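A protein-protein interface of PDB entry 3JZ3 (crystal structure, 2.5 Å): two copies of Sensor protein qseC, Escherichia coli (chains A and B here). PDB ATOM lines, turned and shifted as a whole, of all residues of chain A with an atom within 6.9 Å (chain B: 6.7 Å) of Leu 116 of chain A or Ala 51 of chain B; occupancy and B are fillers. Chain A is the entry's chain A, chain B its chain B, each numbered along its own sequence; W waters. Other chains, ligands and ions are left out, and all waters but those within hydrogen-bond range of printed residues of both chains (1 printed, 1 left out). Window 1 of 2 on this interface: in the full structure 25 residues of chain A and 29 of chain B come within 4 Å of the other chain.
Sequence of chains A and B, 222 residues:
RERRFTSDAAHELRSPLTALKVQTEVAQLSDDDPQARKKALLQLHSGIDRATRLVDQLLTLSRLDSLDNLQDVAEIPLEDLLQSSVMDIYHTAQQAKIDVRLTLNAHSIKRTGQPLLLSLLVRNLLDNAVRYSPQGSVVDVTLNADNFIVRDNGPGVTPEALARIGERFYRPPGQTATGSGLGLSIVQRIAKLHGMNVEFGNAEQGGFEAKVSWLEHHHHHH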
ATOM      1  N   GLN A  43      -4.279 -13.667  15.209  1.00  0.00           N
ATOM      2  CA  GLN A  43      -4.018 -12.291  14.798  1.00  0.00           C
ATOM      3  C   GLN A  43      -3.428 -12.258  13.389  1.00  0.00           C
ATOM      4  O   GLN A  43      -2.381 -12.852  13.129  1.00  0.00           O
ATOM      5  CB  GLN A  43      -3.086 -11.599  15.789  1.00  0.00           C
ATOM      6  CG  GLN A  43      -3.069 -10.090  15.656  1.00  0.00           C
ATOM      7  CD  GLN A  43      -1.829  -9.470  16.262  1.00  0.00           C
ATOM      8  OE1 GLN A  43      -1.285  -9.972  17.246  1.00  0.00           O
ATOM      9  NE2 GLN A  43      -1.374  -8.368  15.677  1.00  0.00           N
ATOM     10  N   VAL A  55       6.370  -1.789  17.622  1.00  0.00           N
ATOM     11  CA  VAL A  55       6.354  -2.194  19.024  1.00  0.00           C
ATOM     12  C   VAL A  55       7.652  -1.804  19.729  1.00  0.00           C
ATOM     13  O   VAL A  55       7.626  -1.310  20.854  1.00  0.00           O
ATOM     14  CB  VAL A  55       6.055  -3.707  19.172  1.00  0.00           C
ATOM     15  CG1 VAL A  55       6.385  -4.196  20.572  1.00  0.00           C
ATOM     16  CG2 VAL A  55       4.595  -3.989  18.841  1.00  0.00           C
ATOM     17  N   ASP A  72      -2.051  -7.907  30.450  1.00  0.00           N
ATOM     18  CA  ASP A  72      -1.970  -9.327  30.077  1.00  0.00           C
ATOM     19  C   ASP A  72      -0.697 -10.081  30.475  1.00  0.00           C
ATOM     20  O   ASP A  72      -0.406 -11.144  29.919  1.00  0.00           O
ATOM     21  CB  ASP A  72      -2.238  -9.514  28.580  1.00  0.00           C
ATOM     22  CG  ASP A  72      -3.635  -9.105  28.183  1.00  0.00           C
ATOM     23  OD1 ASP A  72      -4.594  -9.479  28.896  1.00  0.00           O
ATOM     24  OD2 ASP A  72      -3.771  -8.409  27.153  1.00  0.00           O
ATOM     25  N   ILE A  76       3.538 -17.836  31.564  1.00  0.00           N
ATOM     26  CA  ILE A  76       3.563 -18.424  30.226  1.00  0.00           C
ATOM     27  C   ILE A  76       4.302 -19.762  30.218  1.00  0.00           C
ATOM     28  O   ILE A  76       5.461 -19.827  30.620  1.00  0.00           O
ATOM     29  CB  ILE A  76       4.221 -17.466  29.180  1.00  0.00           C
ATOM     30  CG1 ILE A  76       3.770 -16.009  29.376  1.00  0.00           C
ATOM     31  CG2 ILE A  76       3.976 -17.967  27.748  1.00  0.00           C
ATOM     32  CD1 ILE A  76       2.271 -15.750  29.166  1.00  0.00           C
ATOM     33  N   LEU A  81       4.505 -21.711  23.992  1.00  0.00           N
ATOM     34  CA  LEU A  81       4.949 -20.516  23.276  1.00  0.00           C
ATOM     35  C   LEU A  81       5.845 -20.871  22.097  1.00  0.00           C
ATOM     36  O   LEU A  81       5.632 -20.381  20.987  1.00  0.00           O
ATOM     37  CB  LEU A  81       5.688 -19.556  24.210  1.00  0.00           C
ATOM     38  CG  LEU A  81       6.145 -18.241  23.571  1.00  0.00           C
ATOM     39  CD1 LEU A  81       5.055 -17.187  23.689  1.00  0.00           C
ATOM     40  CD2 LEU A  81       7.428 -17.756  24.221  1.00  0.00           C
ATOM     41  N   GLY A 113       5.443 -13.247  32.028  1.00  0.00           N
ATOM     42  CA  GLY A 113       5.668 -12.380  30.881  1.00  0.00           C
ATOM     43  C   GLY A 113       4.440 -11.956  30.106  1.00  0.00           C
ATOM     44  O   GLY A 113       3.320 -12.394  30.384  1.00  0.00           O
ATOM     45  N   GLN A 114       4.670 -11.081  29.135  1.00  0.00           N
ATOM     46  CA  GLN A 114       3.640 -10.636  28.221  1.00  0.00           C
ATOM     47  C   GLN A 114       3.720 -11.534  26.991  1.00  0.00           C
ATOM     48  O   GLN A 114       4.710 -11.501  26.255  1.00  0.00           O
ATOM     49  CB  GLN A 114       3.836  -9.151  27.893  1.00  0.00           C
ATOM     50  CG  GLN A 114       3.318  -8.706  26.531  1.00  0.00           C
ATOM     51  CD  GLN A 114       1.820  -8.679  26.419  1.00  0.00           C
ATOM     52  OE1 GLN A 114       1.262  -9.184  25.455  1.00  0.00           O
ATOM     53  NE2 GLN A 114       1.156  -8.079  27.397  1.00  0.00           N
ATOM     54  N   PRO A 115       2.686 -12.368  26.783  1.00  0.00           N
ATOM     55  CA  PRO A 115       2.713 -13.406  25.748  1.00  0.00           C
ATOM     56  C   PRO A 115       2.940 -12.865  24.334  1.00  0.00           C
ATOM     57  O   PRO A 115       3.607 -13.519  23.531  1.00  0.00           O
ATOM     58  CB  PRO A 115       1.329 -14.055  25.860  1.00  0.00           C
ATOM     59  CG  PRO A 115       0.493 -13.074  26.603  1.00  0.00           C
ATOM     60  CD  PRO A 115       1.414 -12.367  27.524  1.00  0.00           C
ATOM     61  N   LEU A 116       2.391 -11.687  24.039  1.00  0.00           N
ATOM     62  CA  LEU A 116       2.530 -11.080  22.715  1.00  0.00           C
ATOM     63  C   LEU A 116       3.955 -10.600  22.441  1.00  0.00           C
ATOM     64  O   LEU A 116       4.487 -10.821  21.360  1.00  0.00           O
ATOM     65  CB  LEU A 116       1.532  -9.932  22.546  1.00  0.00           C
ATOM     66  CG  LEU A 116       0.823  -9.804  21.200  1.00  0.00           C
ATOM     67  CD1 LEU A 116      -0.154 -10.961  20.986  1.00  0.00           C
ATOM     68  CD2 LEU A 116       0.098  -8.469  21.118  1.00  0.00           C
ATOM     69  N   LEU A 117       4.573  -9.957  23.428  1.00  0.00           N
ATOM     70  CA  LEU A 117       5.966  -9.530  23.319  1.00  0.00           C
ATOM     71  C   LEU A 117       6.924 -10.712  23.233  1.00  0.00           C
ATOM     72  O   LEU A 117       7.915 -10.661  22.498  1.00  0.00           O
ATOM     73  CB  LEU A 117       6.354  -8.621  24.489  1.00  0.00           C
ATOM     74  CG  LEU A 117       5.646  -7.263  24.586  1.00  0.00           C
ATOM     75  CD1 LEU A 117       6.021  -6.540  25.875  1.00  0.00           C
ATOM     76  CD2 LEU A 117       5.934  -6.389  23.369  1.00  0.00           C
ATOM     77  N   LEU A 118       6.627 -11.772  23.987  1.00  0.00           N
ATOM     78  CA  LEU A 118       7.453 -12.976  23.971  1.00  0.00           C
ATOM     79  C   LEU A 118       7.334 -13.714  22.649  1.00  0.00           C
ATOM     80  O   LEU A 118       8.329 -14.240  22.142  1.00  0.00           O
ATOM     81  CB  LEU A 118       7.106 -13.913  25.129  1.00  0.00           C
ATOM     82  CG  LEU A 118       7.773 -13.666  26.485  1.00  0.00           C
ATOM     83  CD1 LEU A 118       7.356 -14.754  27.457  1.00  0.00           C
ATOM     84  CD2 LEU A 118       9.309 -13.595  26.377  1.00  0.00           C
ATOM     85  N   SER A 119       6.117 -13.746  22.100  1.00  0.00           N
ATOM     86  CA  SER A 119       5.869 -14.346  20.792  1.00  0.00           C
ATOM     87  C   SER A 119       6.635 -13.591  19.722  1.00  0.00           C
ATOM     88  O   SER A 119       7.162 -14.190  18.786  1.00  0.00           O
ATOM     89  CB  SER A 119       4.377 -14.327  20.459  1.00  0.00           C
ATOM     90  OG  SER A 119       3.644 -15.135  21.363  1.00  0.00           O
ATOM     91  N   LEU A 120       6.698 -12.273  19.881  1.00  0.00           N
ATOM     92  CA  LEU A 120       7.373 -11.402  18.939  1.00  0.00           C
ATOM     93  C   LEU A 120       8.875 -11.644  19.004  1.00  0.00           C
ATOM     94  O   LEU A 120       9.551 -11.666  17.974  1.00  0.00           O
ATOM     95  CB  LEU A 120       7.042  -9.943  19.255  1.00  0.00           C
ATOM     96  CG  LEU A 120       6.748  -8.985  18.098  1.00  0.00           C
ATOM     97  CD1 LEU A 120       5.531  -9.426  17.296  1.00  0.00           C
ATOM     98  CD2 LEU A 120       6.532  -7.582  18.635  1.00  0.00           C
ATOM     99  N   LEU A 121       9.382 -11.840  20.221  1.00  0.00           N
ATOM    100  CA  LEU A 121      10.785 -12.180  20.432  1.00  0.00           C
ATOM    101  C   LEU A 121      11.135 -13.476  19.706  1.00  0.00           C
ATOM    102  O   LEU A 121      12.107 -13.528  18.953  1.00  0.00           O
ATOM    103  CB  LEU A 121      11.102 -12.290  21.932  1.00  0.00           C
ATOM    104  CG  LEU A 121      12.545 -12.606  22.353  1.00  0.00           C
ATOM    105  CD1 LEU A 121      12.824 -12.138  23.765  1.00  0.00           C
ATOM    106  CD2 LEU A 121      12.863 -14.090  22.222  1.00  0.00           C
ATOM    107  N   ILE A 190      13.241  -6.942  24.645  1.00  0.00           N
ATOM    108  CA  ILE A 190      12.124  -7.710  25.204  1.00  0.00           C
ATOM    109  C   ILE A 190      12.634  -8.697  26.246  1.00  0.00           C
ATOM    110  O   ILE A 190      11.992  -8.894  27.280  1.00  0.00           O
ATOM    111  CB  ILE A 190      11.298  -8.438  24.098  1.00  0.00           C
ATOM    112  CG1 ILE A 190      10.477  -7.427  23.297  1.00  0.00           C
ATOM    113  CG2 ILE A 190      10.365  -9.497  24.702  1.00  0.00           C
ATOM    114  CD1 ILE A 190       9.871  -7.982  22.026  1.00  0.00           C
ATOM    115  N   LEU B  29      -3.216 -18.293  26.930  1.00  0.00           N
ATOM    116  CA  LEU B  29      -2.662 -16.940  26.899  1.00  0.00           C
ATOM    117  C   LEU B  29      -1.952 -16.644  25.571  1.00  0.00           C
ATOM    118  O   LEU B  29      -1.790 -15.479  25.195  1.00  0.00           O
ATOM    119  CB  LEU B  29      -1.707 -16.724  28.076  1.00  0.00           C
ATOM    120  N   SER B  30      -1.545 -17.703  24.869  1.00  0.00           N
ATOM    121  CA  SER B  30      -0.816 -17.594  23.600  1.00  0.00           C
ATOM    122  C   SER B  30      -1.682 -17.161  22.412  1.00  0.00           C
ATOM    123  O   SER B  30      -2.876 -17.471  22.339  1.00  0.00           O
ATOM    124  CB  SER B  30      -0.085 -18.904  23.274  1.00  0.00           C
ATOM    125  OG  SER B  30       1.105 -19.022  24.034  1.00  0.00           O
ATOM    126  N   ASP B  31      -1.045 -16.451  21.484  1.00  0.00           N
ATOM    127  CA  ASP B  31      -1.703 -15.870  20.321  1.00  0.00           C
ATOM    128  C   ASP B  31      -0.899 -16.181  19.056  1.00  0.00           C
ATOM    129  O   ASP B  31       0.289 -15.860  18.969  1.00  0.00           O
ATOM    130  CB  ASP B  31      -1.843 -14.354  20.525  1.00  0.00           C
ATOM    131  CG  ASP B  31      -2.590 -13.660  19.396  1.00  0.00           C
ATOM    132  OD1 ASP B  31      -2.598 -14.160  18.252  1.00  0.00           O
ATOM    133  OD2 ASP B  31      -3.165 -12.584  19.658  1.00  0.00           O
ATOM    134  N   ASP B  32      -1.558 -16.806  18.083  1.00  0.00           N
ATOM    135  CA  ASP B  32      -0.941 -17.127  16.800  1.00  0.00           C
ATOM    136  C   ASP B  32      -0.797 -15.891  15.906  1.00  0.00           C
ATOM    137  O   ASP B  32      -1.760 -15.152  15.702  1.00  0.00           O
ATOM    138  CB  ASP B  32      -1.747 -18.212  16.079  1.00  0.00           C
ATOM    139  N   ASP B  33       0.414 -15.674  15.390  1.00  0.00           N
ATOM    140  CA  ASP B  33       0.699 -14.589  14.443  1.00  0.00           C
ATOM    141  C   ASP B  33       0.824 -15.121  13.012  1.00  0.00           C
ATOM    142  O   ASP B  33       1.819 -15.769  12.666  1.00  0.00           O
ATOM    143  CB  ASP B  33       1.984 -13.844  14.833  1.00  0.00           C
ATOM    144  CG  ASP B  33       1.857 -13.090  16.148  1.00  0.00           C
ATOM    145  OD1 ASP B  33       0.734 -12.667  16.509  1.00  0.00           O
ATOM    146  OD2 ASP B  33       2.898 -12.911  16.819  1.00  0.00           O
ATOM    147  N   SER B  46     -10.430 -12.022  20.018  1.00  0.00           N
ATOM    148  CA  SER B  46      -9.468 -12.133  21.117  1.00  0.00           C
ATOM    149  C   SER B  46      -8.063 -11.677  20.715  1.00  0.00           C
ATOM    150  O   SER B  46      -7.393 -10.984  21.481  1.00  0.00           O
ATOM    151  CB  SER B  46      -9.432 -13.571  21.646  1.00  0.00           C
ATOM    152  OG  SER B  46      -8.339 -13.773  22.524  1.00  0.00           O
ATOM    153  N   GLY B  47      -7.629 -12.073  19.519  1.00  0.00           N
ATOM    154  CA  GLY B  47      -6.339 -11.650  18.974  1.00  0.00           C
ATOM    155  C   GLY B  47      -6.223 -10.141  18.880  1.00  0.00           C
ATOM    156  O   GLY B  47      -5.234  -9.553  19.328  1.00  0.00           O
ATOM    157  N   ILE B  48      -7.248  -9.519  18.301  1.00  0.00           N
ATOM    158  CA  ILE B  48      -7.338  -8.061  18.185  1.00  0.00           C
ATOM    159  C   ILE B  48      -7.466  -7.394  19.553  1.00  0.00           C
ATOM    160  O   ILE B  48      -6.921  -6.312  19.775  1.00  0.00           O
ATOM    161  CB  ILE B  48      -8.511  -7.648  17.249  1.00  0.00           C
ATOM    162  CG1 ILE B  48      -8.171  -7.978  15.786  1.00  0.00           C
ATOM    163  CG2 ILE B  48      -8.899  -6.169  17.421  1.00  0.00           C
ATOM    164  CD1 ILE B  48      -6.899  -7.298  15.232  1.00  0.00           C
ATOM    165  N   ASP B  49      -8.170  -8.059  20.465  1.00  0.00           N
ATOM    166  CA  ASP B  49      -8.376  -7.569  21.824  1.00  0.00           C
ATOM    167  C   ASP B  49      -7.066  -7.480  22.613  1.00  0.00           C
ATOM    168  O   ASP B  49      -6.840  -6.514  23.344  1.00  0.00           O
ATOM    169  CB  ASP B  49      -9.353  -8.491  22.554  1.00  0.00           C
ATOM    170  CG  ASP B  49     -10.562  -7.756  23.077  1.00  0.00           C
ATOM    171  OD1 ASP B  49     -10.398  -6.918  23.991  1.00  0.00           O
ATOM    172  OD2 ASP B  49     -11.678  -8.024  22.571  1.00  0.00           O
ATOM    173  N   ARG B  50      -6.219  -8.494  22.456  1.00  0.00           N
ATOM    174  CA  ARG B  50      -4.928  -8.553  23.139  1.00  0.00           C
ATOM    175  C   ARG B  50      -3.917  -7.563  22.565  1.00  0.00           C
ATOM    176  O   ARG B  50      -3.199  -6.908  23.315  1.00  0.00           O
ATOM    177  CB  ARG B  50      -4.358  -9.968  23.082  1.00  0.00           C
ATOM    178  CG  ARG B  50      -5.136 -10.974  23.900  1.00  0.00           C
ATOM    179  CD  ARG B  50      -4.787 -12.379  23.475  1.00  0.00           C
ATOM    180  NE  ARG B  50      -5.577 -13.360  24.204  1.00  0.00           N
ATOM    181  CZ  ARG B  50      -5.362 -14.670  24.181  1.00  0.00           C
ATOM    182  NH1 ARG B  50      -4.370 -15.180  23.458  1.00  0.00           N
ATOM    183  NH2 ARG B  50      -6.145 -15.472  24.890  1.00  0.00           N
ATOM    184  N   ALA B  51      -3.866  -7.463  21.238  1.00  0.00           N
ATOM    185  CA  ALA B  51      -3.006  -6.491  20.565  1.00  0.00           C
ATOM    186  C   ALA B  51      -3.431  -5.062  20.889  1.00  0.00           C
ATOM    187  O   ALA B  51      -2.583  -4.188  21.081  1.00  0.00           O
ATOM    188  CB  ALA B  51      -3.006  -6.722  19.066  1.00  0.00           C
ATOM    189  N   THR B  52      -4.744  -4.842  20.963  1.00  0.00           N
ATOM    190  CA  THR B  52      -5.322  -3.542  21.315  1.00  0.00           C
ATOM    191  C   THR B  52      -4.893  -3.104  22.714  1.00  0.00           C
ATOM    192  O   THR B  52      -4.338  -2.020  22.881  1.00  0.00           O
ATOM    193  CB  THR B  52      -6.870  -3.571  21.219  1.00  0.00           C
ATOM    194  OG1 THR B  52      -7.259  -3.698  19.847  1.00  0.00           O
ATOM    195  CG2 THR B  52      -7.492  -2.308  21.800  1.00  0.00           C
ATOM    196  N   ARG B  53      -5.149  -3.958  23.705  1.00  0.00           N
ATOM    197  CA  ARG B  53      -4.772  -3.700  25.098  1.00  0.00           C
ATOM    198  C   ARG B  53      -3.303  -3.310  25.273  1.00  0.00           C
ATOM    199  O   ARG B  53      -2.996  -2.318  25.943  1.00  0.00           O
ATOM    200  CB  ARG B  53      -5.119  -4.907  25.971  1.00  0.00           C
ATOM    201  CG  ARG B  53      -6.323  -4.678  26.865  1.00  0.00           C
ATOM    202  CD  ARG B  53      -7.316  -5.830  26.824  1.00  0.00           C
ATOM    203  NE  ARG B  53      -6.732  -7.140  27.111  1.00  0.00           N
ATOM    204  CZ  ARG B  53      -7.340  -8.298  26.848  1.00  0.00           C
ATOM    205  NH1 ARG B  53      -8.548  -8.313  26.289  1.00  0.00           N
ATOM    206  NH2 ARG B  53      -6.741  -9.443  27.134  1.00  0.00           N
ATOM    207  N   LEU B  54      -2.404  -4.074  24.656  1.00  0.00           N
ATOM    208  CA  LEU B  54      -0.970  -3.808  24.745  1.00  0.00           C
ATOM    209  C   LEU B  54      -0.575  -2.490  24.076  1.00  0.00           C
ATOM    210  O   LEU B  54       0.084  -1.650  24.698  1.00  0.00           O
ATOM    211  CB  LEU B  54      -0.165  -4.972  24.151  1.00  0.00           C
ATOM    212  CG  LEU B  54       1.368  -4.896  24.195  1.00  0.00           C
ATOM    213  CD1 LEU B  54       1.894  -4.693  25.618  1.00  0.00           C
ATOM    214  CD2 LEU B  54       1.975  -6.145  23.574  1.00  0.00           C
ATOM    215  N   VAL B  55      -0.980  -2.315  22.818  1.00  0.00           N
ATOM    216  CA  VAL B  55      -0.591  -1.144  22.030  1.00  0.00           C
ATOM    217  C   VAL B  55      -1.253   0.128  22.565  1.00  0.00           C
ATOM    218  O   VAL B  55      -0.638   1.197  22.564  1.00  0.00           O
ATOM    219  CB  VAL B  55      -0.860  -1.345  20.510  1.00  0.00           C
ATOM    220  CG1 VAL B  55      -0.590  -0.069  19.731  1.00  0.00           C
ATOM    221  CG2 VAL B  55       0.003  -2.480  19.961  1.00  0.00           C
ATOM    222  N   ASP B  56      -2.494   0.003  23.038  1.00  0.00           N
ATOM    223  CA  ASP B  56      -3.177   1.104  23.718  1.00  0.00           C
ATOM    224  C   ASP B  56      -2.374   1.592  24.919  1.00  0.00           C
ATOM    225  O   ASP B  56      -2.136   2.792  25.064  1.00  0.00           O
ATOM    226  CB  ASP B  56      -4.582   0.689  24.166  1.00  0.00           C
ATOM    227  CG  ASP B  56      -5.374   1.840  24.781  1.00  0.00           C
ATOM    228  OD1 ASP B  56      -5.187   3.007  24.368  1.00  0.00           O
ATOM    229  OD2 ASP B  56      -6.197   1.571  25.681  1.00  0.00           O
ATOM    230  N   LEU B 120      -5.694  -1.514  13.326  1.00  0.00           N
ATOM    231  CA  LEU B 120      -6.238  -1.792  14.660  1.00  0.00           C
ATOM    232  C   LEU B 120      -7.520  -1.018  14.931  1.00  0.00           C
ATOM    233  O   LEU B 120      -8.493  -1.585  15.421  1.00  0.00           O
ATOM    234  CB  LEU B 120      -5.213  -1.456  15.750  1.00  0.00           C
ATOM    235  CG  LEU B 120      -4.128  -2.476  16.087  1.00  0.00           C
ATOM    236  CD1 LEU B 120      -3.149  -1.867  17.078  1.00  0.00           C
ATOM    237  CD2 LEU B 120      -4.733  -3.761  16.645  1.00  0.00           C
ATOM    238  N   ILE B 186      -9.216   3.157  22.440  1.00  0.00           N
ATOM    239  CA  ILE B 186      -8.006   3.169  21.621  1.00  0.00           C
ATOM    240  C   ILE B 186      -8.365   3.734  20.247  1.00  0.00           C
ATOM    241  O   ILE B 186      -7.538   4.381  19.592  1.00  0.00           O
ATOM    242  CB  ILE B 186      -7.370   1.752  21.486  1.00  0.00           C
ATOM    243  CG1 ILE B 186      -5.933   1.858  20.949  1.00  0.00           C
ATOM    244  CG2 ILE B 186      -8.247   0.832  20.628  1.00  0.00           C
ATOM    245  CD1 ILE B 186      -5.269   0.522  20.589  1.00  0.00           C
HETATM  246  O   HOH W   1       1.049 -14.805  22.153  1.00  0.00           O
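Positions printed for both chains: 55 and 120.
OD1 of Asp 31 of chain B touches N of Gln 43 of chain A, 3.5 Å away.
OE1 of Gln 114 of chain A touches CD2 of Leu 54 of chain B (3.6 Å).
CB of Pro 115 of chain A touches O of Leu 29 of chain B (3.5 Å).
Asp 31 of chain B touches Leu 116 of chain A (OD2 to CD1, 3.7 Å).
Leu 116 of chain A touches Ala 51 of chain B.
CD2 of Leu 54 of chain B touches CD2 of Leu 116 of chain A (3.9 Å).
CG of Leu 117 of chain A touches CD2 of Leu 54 of chain B (3.97 Å).
Water W1 lies within hydrogen-bond range of OG of Ser 119 of chain A (2.7 Å), N of Asp 31 of chain B (2.7 Å) and O of Pro 115 of chain A (3.2 Å).
The side-chain carboxylate (OD1) of Asp 72 of chain A lies within salt-bridge range of the guanidinium group (NH2) of Arg 53 of chain B (2.8 Å).
The side-chain carboxylate of Asp 33 of chain B sits close to the side-chain amide oxygen of Gln 43 of chain A (3.4 Å).
The backbone NH of Gln 43 of chain A lies within hydrogen-bond range of the backbone carbonyl oxygen of Asp 32 of chain B (3.0 Å).
Printed residues of chain B within 4 Å of Pro 115 of chain A: Leu 29.
Of chain B, only Asp 31 (3.7 Å), Ala 51 (3.7 Å) and Leu 54 (3.9 Å) come within 4 Å of Leu 116 of chain A.
Ile 190 of chain A touches none of the printed residues of chain B.
Of chain A, only Leu 116 comes within 4 Å of Ala 51 of chain B.
Of the printed residues of chain A, Arg 53 of chain B touches Asp 72 (2.8 Å).
Val 55 of chain B touches none of the printed residues of chain A.
The nearest residue of chain A that does not touch Ala 51 of chain B is Gln 43 of chain A (4.1 Å).
The nearest printed residue of chain B that does not touch Asp 72 of chain A is Arg 50 of chain B (4.2 Å).
Of the 18 printed residues of chain B, 7 touch a printed residue of chain A.
Of the 15 printed residues of chain A, 6 touch a printed residue of chain B.
Hydrophobic or aromatic side chains of chain A that line the printed part of chain B: Pro 115, Leu 116 and Leu 117.
Among the printed residues, 10 pairs touch across the chains.
Among the printed residues, Asp or Glu carboxylates within 4 Å of a Lys or Arg side-chain nitrogen of the other chain: Asp 72 of chain A with Arg 53 of chain B.
NH1 of Arg 50 of chain B lies within hydrogen-bond range of O of Leu 29 of chain B, 3.1 Å away.
The side-chain amide oxygen (OE1) of Gln 114 of chain A sits close to the backbone NH (N) of Leu 116 of chain A, at 3.1 Å.
The backbone carbonyl oxygen of Pro 115 of chain A sits at hydrogen-bond distance from the side-chain hydroxyl of Ser 119 of chain A, at 2.7 Å.
The guanidinium group (NH1) of Arg 53 of chain B is in salt-bridge range of the side-chain carboxylate (OD1) of Asp 49 of chain B (3.3 Å).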
